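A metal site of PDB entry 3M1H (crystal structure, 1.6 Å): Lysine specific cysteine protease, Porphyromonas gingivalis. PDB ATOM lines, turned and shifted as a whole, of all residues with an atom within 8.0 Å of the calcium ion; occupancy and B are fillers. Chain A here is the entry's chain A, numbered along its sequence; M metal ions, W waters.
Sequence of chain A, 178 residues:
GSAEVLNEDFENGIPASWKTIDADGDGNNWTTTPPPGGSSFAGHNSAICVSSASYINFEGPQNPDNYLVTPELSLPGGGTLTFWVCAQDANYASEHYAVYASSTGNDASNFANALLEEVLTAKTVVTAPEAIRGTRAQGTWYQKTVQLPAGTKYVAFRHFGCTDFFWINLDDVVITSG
N of Asp 24 lies within hydrogen-bond range of O of Asp 65. ND2 of Asn 66 lies within hydrogen-bond range of OG of Ser 52. The backbone NH of Gly 27 is in hydrogen-bond range of the side-chain carboxylate of Asp 22, at 2.8 Å. OE1 of Gln 62 lies close to OD2 of Asp 26 (3.3 Å). The indole nitrogen (NE1) of Trp 30 sits at hydrogen-bond distance from the backbone carbonyl oxygen (O) of Asn 66 (3.0 Å). N of His 159 is in hydrogen-bond range of O of Asn 66 (2.9 Å). ND2 of Asn 28 sits at hydrogen-bond distance from OE1 of Gln 62 (3.1 Å). N of Gly 25 sits close to OD1 of Asp 22 (3.2 Å).
Of the 19 residues printed, 5 come within 4 Å of the calcium ion. The nearest printed residue that does not touch the calcium ion is Asp 65 (4.5 Å).
The calcium ion is bound by OD1 of Asp 22 (2.3 Å), OD1 of Asn 66 (2.4 Å), O of Asn 28 (2.4 Å), water W1 (2.4 Å), OD1 of Asp 26 (2.4 Å), OD1 of Asp 24 (2.4 Å) and OD2 of Asp 24 (2.8 Å). The calcium ion has seven donor atoms within binding distance.
Water W1 lies within hydrogen-bond range of the side-chain carboxylate of Asp 26 (2.7 Å) and the side-chain amide nitrogen of Asn 66 (3.4 Å).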
ATOM      1  N   ILE A  21     -16.823   3.047 -12.282  1.00  0.00           N
ATOM      2  CA  ILE A  21     -16.245   1.889 -11.585  1.00  0.00           C
ATOM      3  C   ILE A  21     -16.188   2.229 -10.082  1.00  0.00           C
ATOM      4  O   ILE A  21     -15.549   3.199  -9.691  1.00  0.00           O
ATOM      5  CB  ILE A  21     -14.837   1.523 -12.084  1.00  0.00           C
ATOM      6  CG1 ILE A  21     -14.826   1.252 -13.583  1.00  0.00           C
ATOM      7  CG2 ILE A  21     -14.375   0.253 -11.348  1.00  0.00           C
ATOM      8  CD1 ILE A  21     -13.421   1.093 -14.144  1.00  0.00           C
ATOM      9  N   ASP A  22     -16.912   1.444  -9.276  1.00  0.00           N
ATOM     10  CA  ASP A  22     -16.878   1.586  -7.809  1.00  0.00           C
ATOM     11  C   ASP A  22     -15.824   0.624  -7.241  1.00  0.00           C
ATOM     12  O   ASP A  22     -16.156  -0.493  -6.802  1.00  0.00           O
ATOM     13  CB  ASP A  22     -18.254   1.288  -7.212  1.00  0.00           C
ATOM     14  CG  ASP A  22     -18.304   1.467  -5.739  1.00  0.00           C
ATOM     15  OD1 ASP A  22     -17.359   2.075  -5.126  1.00  0.00           O
ATOM     16  OD2 ASP A  22     -19.301   0.975  -5.167  1.00  0.00           O
ATOM     17  N   ALA A  23     -14.557   1.018  -7.309  1.00  0.00           N
ATOM     18  CA  ALA A  23     -13.475   0.081  -6.926  1.00  0.00           C
ATOM     19  C   ALA A  23     -13.410  -0.191  -5.439  1.00  0.00           C
ATOM     20  O   ALA A  23     -13.089  -1.326  -5.045  1.00  0.00           O
ATOM     21  CB  ALA A  23     -12.097   0.477  -7.490  1.00  0.00           C
ATOM     22  N   ASP A  24     -13.768   0.771  -4.596  1.00  0.00           N
ATOM     23  CA  ASP A  24     -13.783   0.509  -3.159  1.00  0.00           C
ATOM     24  C   ASP A  24     -15.014  -0.299  -2.682  1.00  0.00           C
ATOM     25  O   ASP A  24     -14.998  -0.912  -1.595  1.00  0.00           O
ATOM     26  CB  ASP A  24     -13.728   1.827  -2.400  1.00  0.00           C
ATOM     27  CG  ASP A  24     -14.897   2.704  -2.739  1.00  0.00           C
ATOM     28  OD1 ASP A  24     -14.797   3.354  -3.835  1.00  0.00           O
ATOM     29  OD2 ASP A  24     -15.902   2.721  -1.991  1.00  0.00           O
ATOM     30  N   GLY A  25     -16.075  -0.298  -3.462  1.00  0.00           N
ATOM     31  CA  GLY A  25     -17.233  -1.156  -3.224  1.00  0.00           C
ATOM     32  C   GLY A  25     -18.309  -0.636  -2.300  1.00  0.00           C
ATOM     33  O   GLY A  25     -19.204  -1.395  -1.904  1.00  0.00           O
ATOM     34  N   ASP A  26     -18.265   0.651  -1.936  1.00  0.00           N
ATOM     35  CA  ASP A  26     -19.239   1.195  -0.986  1.00  0.00           C
ATOM     36  C   ASP A  26     -20.604   1.572  -1.520  1.00  0.00           C
ATOM     37  O   ASP A  26     -21.498   1.977  -0.764  1.00  0.00           O
ATOM     38  CB  ASP A  26     -18.645   2.391  -0.219  1.00  0.00           C
ATOM     39  CG  ASP A  26     -18.474   3.628  -1.071  1.00  0.00           C
ATOM     40  OD1 ASP A  26     -18.645   3.529  -2.326  1.00  0.00           O
ATOM     41  OD2 ASP A  26     -18.132   4.676  -0.475  1.00  0.00           O
ATOM     42  N   GLY A  27     -20.775   1.471  -2.846  1.00  0.00           N
ATOM     43  CA  GLY A  27     -21.995   1.880  -3.531  1.00  0.00           C
ATOM     44  C   GLY A  27     -22.074   3.312  -3.985  1.00  0.00           C
ATOM     45  O   GLY A  27     -23.008   3.687  -4.691  1.00  0.00           O
ATOM     46  N   ASN A  28     -21.108   4.111  -3.576  1.00  0.00           N
ATOM     47  CA  ASN A  28     -21.004   5.523  -3.938  1.00  0.00           C
ATOM     48  C   ASN A  28     -20.055   5.656  -5.128  1.00  0.00           C
ATOM     49  O   ASN A  28     -18.944   5.106  -5.167  1.00  0.00           O
ATOM     50  CB  ASN A  28     -20.469   6.334  -2.749  1.00  0.00           C
ATOM     51  CG  ASN A  28     -21.435   6.359  -1.584  1.00  0.00           C
ATOM     52  OD1 ASN A  28     -22.607   6.689  -1.750  1.00  0.00           O
ATOM     53  ND2 ASN A  28     -20.943   6.037  -0.395  1.00  0.00           N
ATOM     54  N   ASN A  29     -20.504   6.445  -6.119  1.00  0.00           N
ATOM     55  CA  ASN A  29     -19.772   6.626  -7.360  1.00  0.00           C
ATOM     56  C   ASN A  29     -19.635   8.099  -7.717  1.00  0.00           C
ATOM     57  O   ASN A  29     -20.209   8.984  -7.097  1.00  0.00           O
ATOM     58  CB  ASN A  29     -20.554   5.943  -8.488  1.00  0.00           C
ATOM     59  CG  ASN A  29     -20.438   4.426  -8.463  1.00  0.00           C
ATOM     60  OD1 ASN A  29     -19.429   3.863  -8.904  1.00  0.00           O
ATOM     61  ND2 ASN A  29     -21.473   3.753  -7.949  1.00  0.00           N
ATOM     62  N   TRP A  30     -18.951   8.316  -8.831  1.00  0.00           N
ATOM     63  CA  TRP A  30     -19.126   9.574  -9.526  1.00  0.00           C
ATOM     64  C   TRP A  30     -20.613   9.629  -9.895  1.00  0.00           C
ATOM     65  O   TRP A  30     -21.201   8.636 -10.342  1.00  0.00           O
ATOM     66  CB  TRP A  30     -18.299   9.616 -10.791  1.00  0.00           C
ATOM     67  CG  TRP A  30     -16.826   9.832 -10.608  1.00  0.00           C
ATOM     68  CD1 TRP A  30     -15.879   8.878 -10.527  1.00  0.00           C
ATOM     69  CD2 TRP A  30     -16.142  11.099 -10.516  1.00  0.00           C
ATOM     70  NE1 TRP A  30     -14.631   9.450 -10.375  1.00  0.00           N
ATOM     71  CE2 TRP A  30     -14.767  10.812 -10.380  1.00  0.00           C
ATOM     72  CE3 TRP A  30     -16.567  12.431 -10.547  1.00  0.00           C
ATOM     73  CZ2 TRP A  30     -13.819  11.815 -10.289  1.00  0.00           C
ATOM     74  CZ3 TRP A  30     -15.619  13.434 -10.441  1.00  0.00           C
ATOM     75  CH2 TRP A  30     -14.272  13.116 -10.290  1.00  0.00           C
ATOM     76  N   SER A  52     -17.750  13.341  -7.095  1.00  0.00           N
ATOM     77  CA  SER A  52     -17.433  12.168  -6.261  1.00  0.00           C
ATOM     78  C   SER A  52     -17.072  12.627  -4.841  1.00  0.00           C
ATOM     79  O   SER A  52     -16.418  13.626  -4.677  1.00  0.00           O
ATOM     80  CB  SER A  52     -16.343  11.358  -6.908  1.00  0.00           C
ATOM     81  OG  SER A  52     -15.868  10.247  -6.098  1.00  0.00           O
ATOM     82  N   ALA A  53     -17.520  11.861  -3.846  1.00  0.00           N
ATOM     83  CA  ALA A  53     -17.426  12.269  -2.437  1.00  0.00           C
ATOM     84  C   ALA A  53     -16.318  11.617  -1.666  1.00  0.00           C
ATOM     85  O   ALA A  53     -16.117  10.410  -1.723  1.00  0.00           O
ATOM     86  CB  ALA A  53     -18.752  11.966  -1.706  1.00  0.00           C
ATOM     87  N   GLN A  62     -16.084   9.224   3.641  1.00  0.00           N
ATOM     88  CA  GLN A  62     -16.018   8.100   2.712  1.00  0.00           C
ATOM     89  C   GLN A  62     -14.560   7.816   2.352  1.00  0.00           C
ATOM     90  O   GLN A  62     -13.678   8.665   2.562  1.00  0.00           O
ATOM     91  CB  GLN A  62     -16.799   8.444   1.433  1.00  0.00           C
ATOM     92  CG  GLN A  62     -18.171   8.927   1.687  1.00  0.00           C
ATOM     93  CD  GLN A  62     -19.045   7.875   2.340  1.00  0.00           C
ATOM     94  OE1 GLN A  62     -19.036   6.716   1.929  1.00  0.00           O
ATOM     95  NE2 GLN A  62     -19.769   8.270   3.357  1.00  0.00           N
ATOM     96  N   ASN A  63     -14.305   6.635   1.807  1.00  0.00           N
ATOM     97  CA  ASN A  63     -13.002   6.239   1.309  1.00  0.00           C
ATOM     98  C   ASN A  63     -13.084   5.877  -0.165  1.00  0.00           C
ATOM     99  O   ASN A  63     -13.011   4.703  -0.554  1.00  0.00           O
ATOM    100  CB  ASN A  63     -12.460   5.090   2.155  1.00  0.00           C
ATOM    101  CG  ASN A  63     -12.207   5.529   3.584  1.00  0.00           C
ATOM    102  OD1 ASN A  63     -11.167   6.119   3.892  1.00  0.00           O
ATOM    103  ND2 ASN A  63     -13.179   5.319   4.444  1.00  0.00           N
ATOM    104  N   PRO A  64     -13.274   6.897  -1.015  1.00  0.00           N
ATOM    105  CA  PRO A  64     -13.534   6.603  -2.427  1.00  0.00           C
ATOM    106  C   PRO A  64     -12.342   5.996  -3.151  1.00  0.00           C
ATOM    107  O   PRO A  64     -11.171   6.333  -2.899  1.00  0.00           O
ATOM    108  CB  PRO A  64     -13.907   7.993  -2.991  1.00  0.00           C
ATOM    109  CG  PRO A  64     -13.188   8.979  -2.077  1.00  0.00           C
ATOM    110  CD  PRO A  64     -13.323   8.341  -0.720  1.00  0.00           C
ATOM    111  N   ASP A  65     -12.669   5.083  -4.062  1.00  0.00           N
ATOM    112  CA  ASP A  65     -11.785   4.704  -5.152  1.00  0.00           C
ATOM    113  C   ASP A  65     -12.734   4.547  -6.330  1.00  0.00           C
ATOM    114  O   ASP A  65     -13.142   3.437  -6.690  1.00  0.00           O
ATOM    115  CB  ASP A  65     -10.968   3.432  -4.856  1.00  0.00           C
ATOM    116  CG  ASP A  65      -9.904   3.151  -5.921  1.00  0.00           C
ATOM    117  OD1 ASP A  65      -9.819   3.875  -6.934  1.00  0.00           O
ATOM    118  OD2 ASP A  65      -9.124   2.204  -5.783  1.00  0.00           O
ATOM    119  N   ASN A  66     -13.119   5.693  -6.873  1.00  0.00           N
ATOM    120  CA  ASN A  66     -14.171   5.803  -7.875  1.00  0.00           C
ATOM    121  C   ASN A  66     -13.597   6.244  -9.200  1.00  0.00           C
ATOM    122  O   ASN A  66     -12.926   7.261  -9.284  1.00  0.00           O
ATOM    123  CB  ASN A  66     -15.211   6.836  -7.448  1.00  0.00           C
ATOM    124  CG  ASN A  66     -15.915   6.503  -6.160  1.00  0.00           C
ATOM    125  OD1 ASN A  66     -15.955   5.350  -5.708  1.00  0.00           O
ATOM    126  ND2 ASN A  66     -16.503   7.535  -5.545  1.00  0.00           N
ATOM    127  N   TYR A  67     -13.902   5.491 -10.258  1.00  0.00           N
ATOM    128  CA  TYR A  67     -13.505   5.875 -11.637  1.00  0.00           C
ATOM    129  C   TYR A  67     -14.701   6.302 -12.450  1.00  0.00           C
ATOM    130  O   TYR A  67     -15.806   5.766 -12.300  1.00  0.00           O
ATOM    131  CB  TYR A  67     -12.820   4.743 -12.406  1.00  0.00           C
ATOM    132  CG  TYR A  67     -11.601   4.116 -11.757  1.00  0.00           C
ATOM    133  CD1 TYR A  67     -10.374   4.226 -12.368  1.00  0.00           C
ATOM    134  CD2 TYR A  67     -11.688   3.354 -10.587  1.00  0.00           C
ATOM    135  CE1 TYR A  67      -9.222   3.602 -11.825  1.00  0.00           C
ATOM    136  CE2 TYR A  67     -10.539   2.742 -10.037  1.00  0.00           C
ATOM    137  CZ  TYR A  67      -9.317   2.875 -10.677  1.00  0.00           C
ATOM    138  OH  TYR A  67      -8.154   2.277 -10.191  1.00  0.00           O
ATOM    139  N   HIS A 159     -11.037   9.280  -8.415  1.00  0.00           N
ATOM    140  CA  HIS A 159     -11.056   9.982  -7.135  1.00  0.00           C
ATOM    141  C   HIS A 159     -10.700   8.941  -6.079  1.00  0.00           C
ATOM    142  O   HIS A 159     -11.416   7.945  -5.960  1.00  0.00           O
ATOM    143  CB  HIS A 159     -12.452  10.498  -6.860  1.00  0.00           C
ATOM    144  CG  HIS A 159     -12.597  11.318  -5.604  1.00  0.00           C
ATOM    145  ND1 HIS A 159     -13.757  11.368  -4.885  1.00  0.00           N
ATOM    146  CD2 HIS A 159     -11.713  12.127  -4.947  1.00  0.00           C
ATOM    147  CE1 HIS A 159     -13.627  12.216  -3.871  1.00  0.00           C
ATOM    148  NE2 HIS A 159     -12.393  12.680  -3.885  1.00  0.00           N
HETATM  149 CA    CA M   1     -17.099   4.097  -4.064  1.00  0.00          CA
HETATM  150  O   HOH W   1     -16.871   5.909  -2.543  1.00  0.00           O
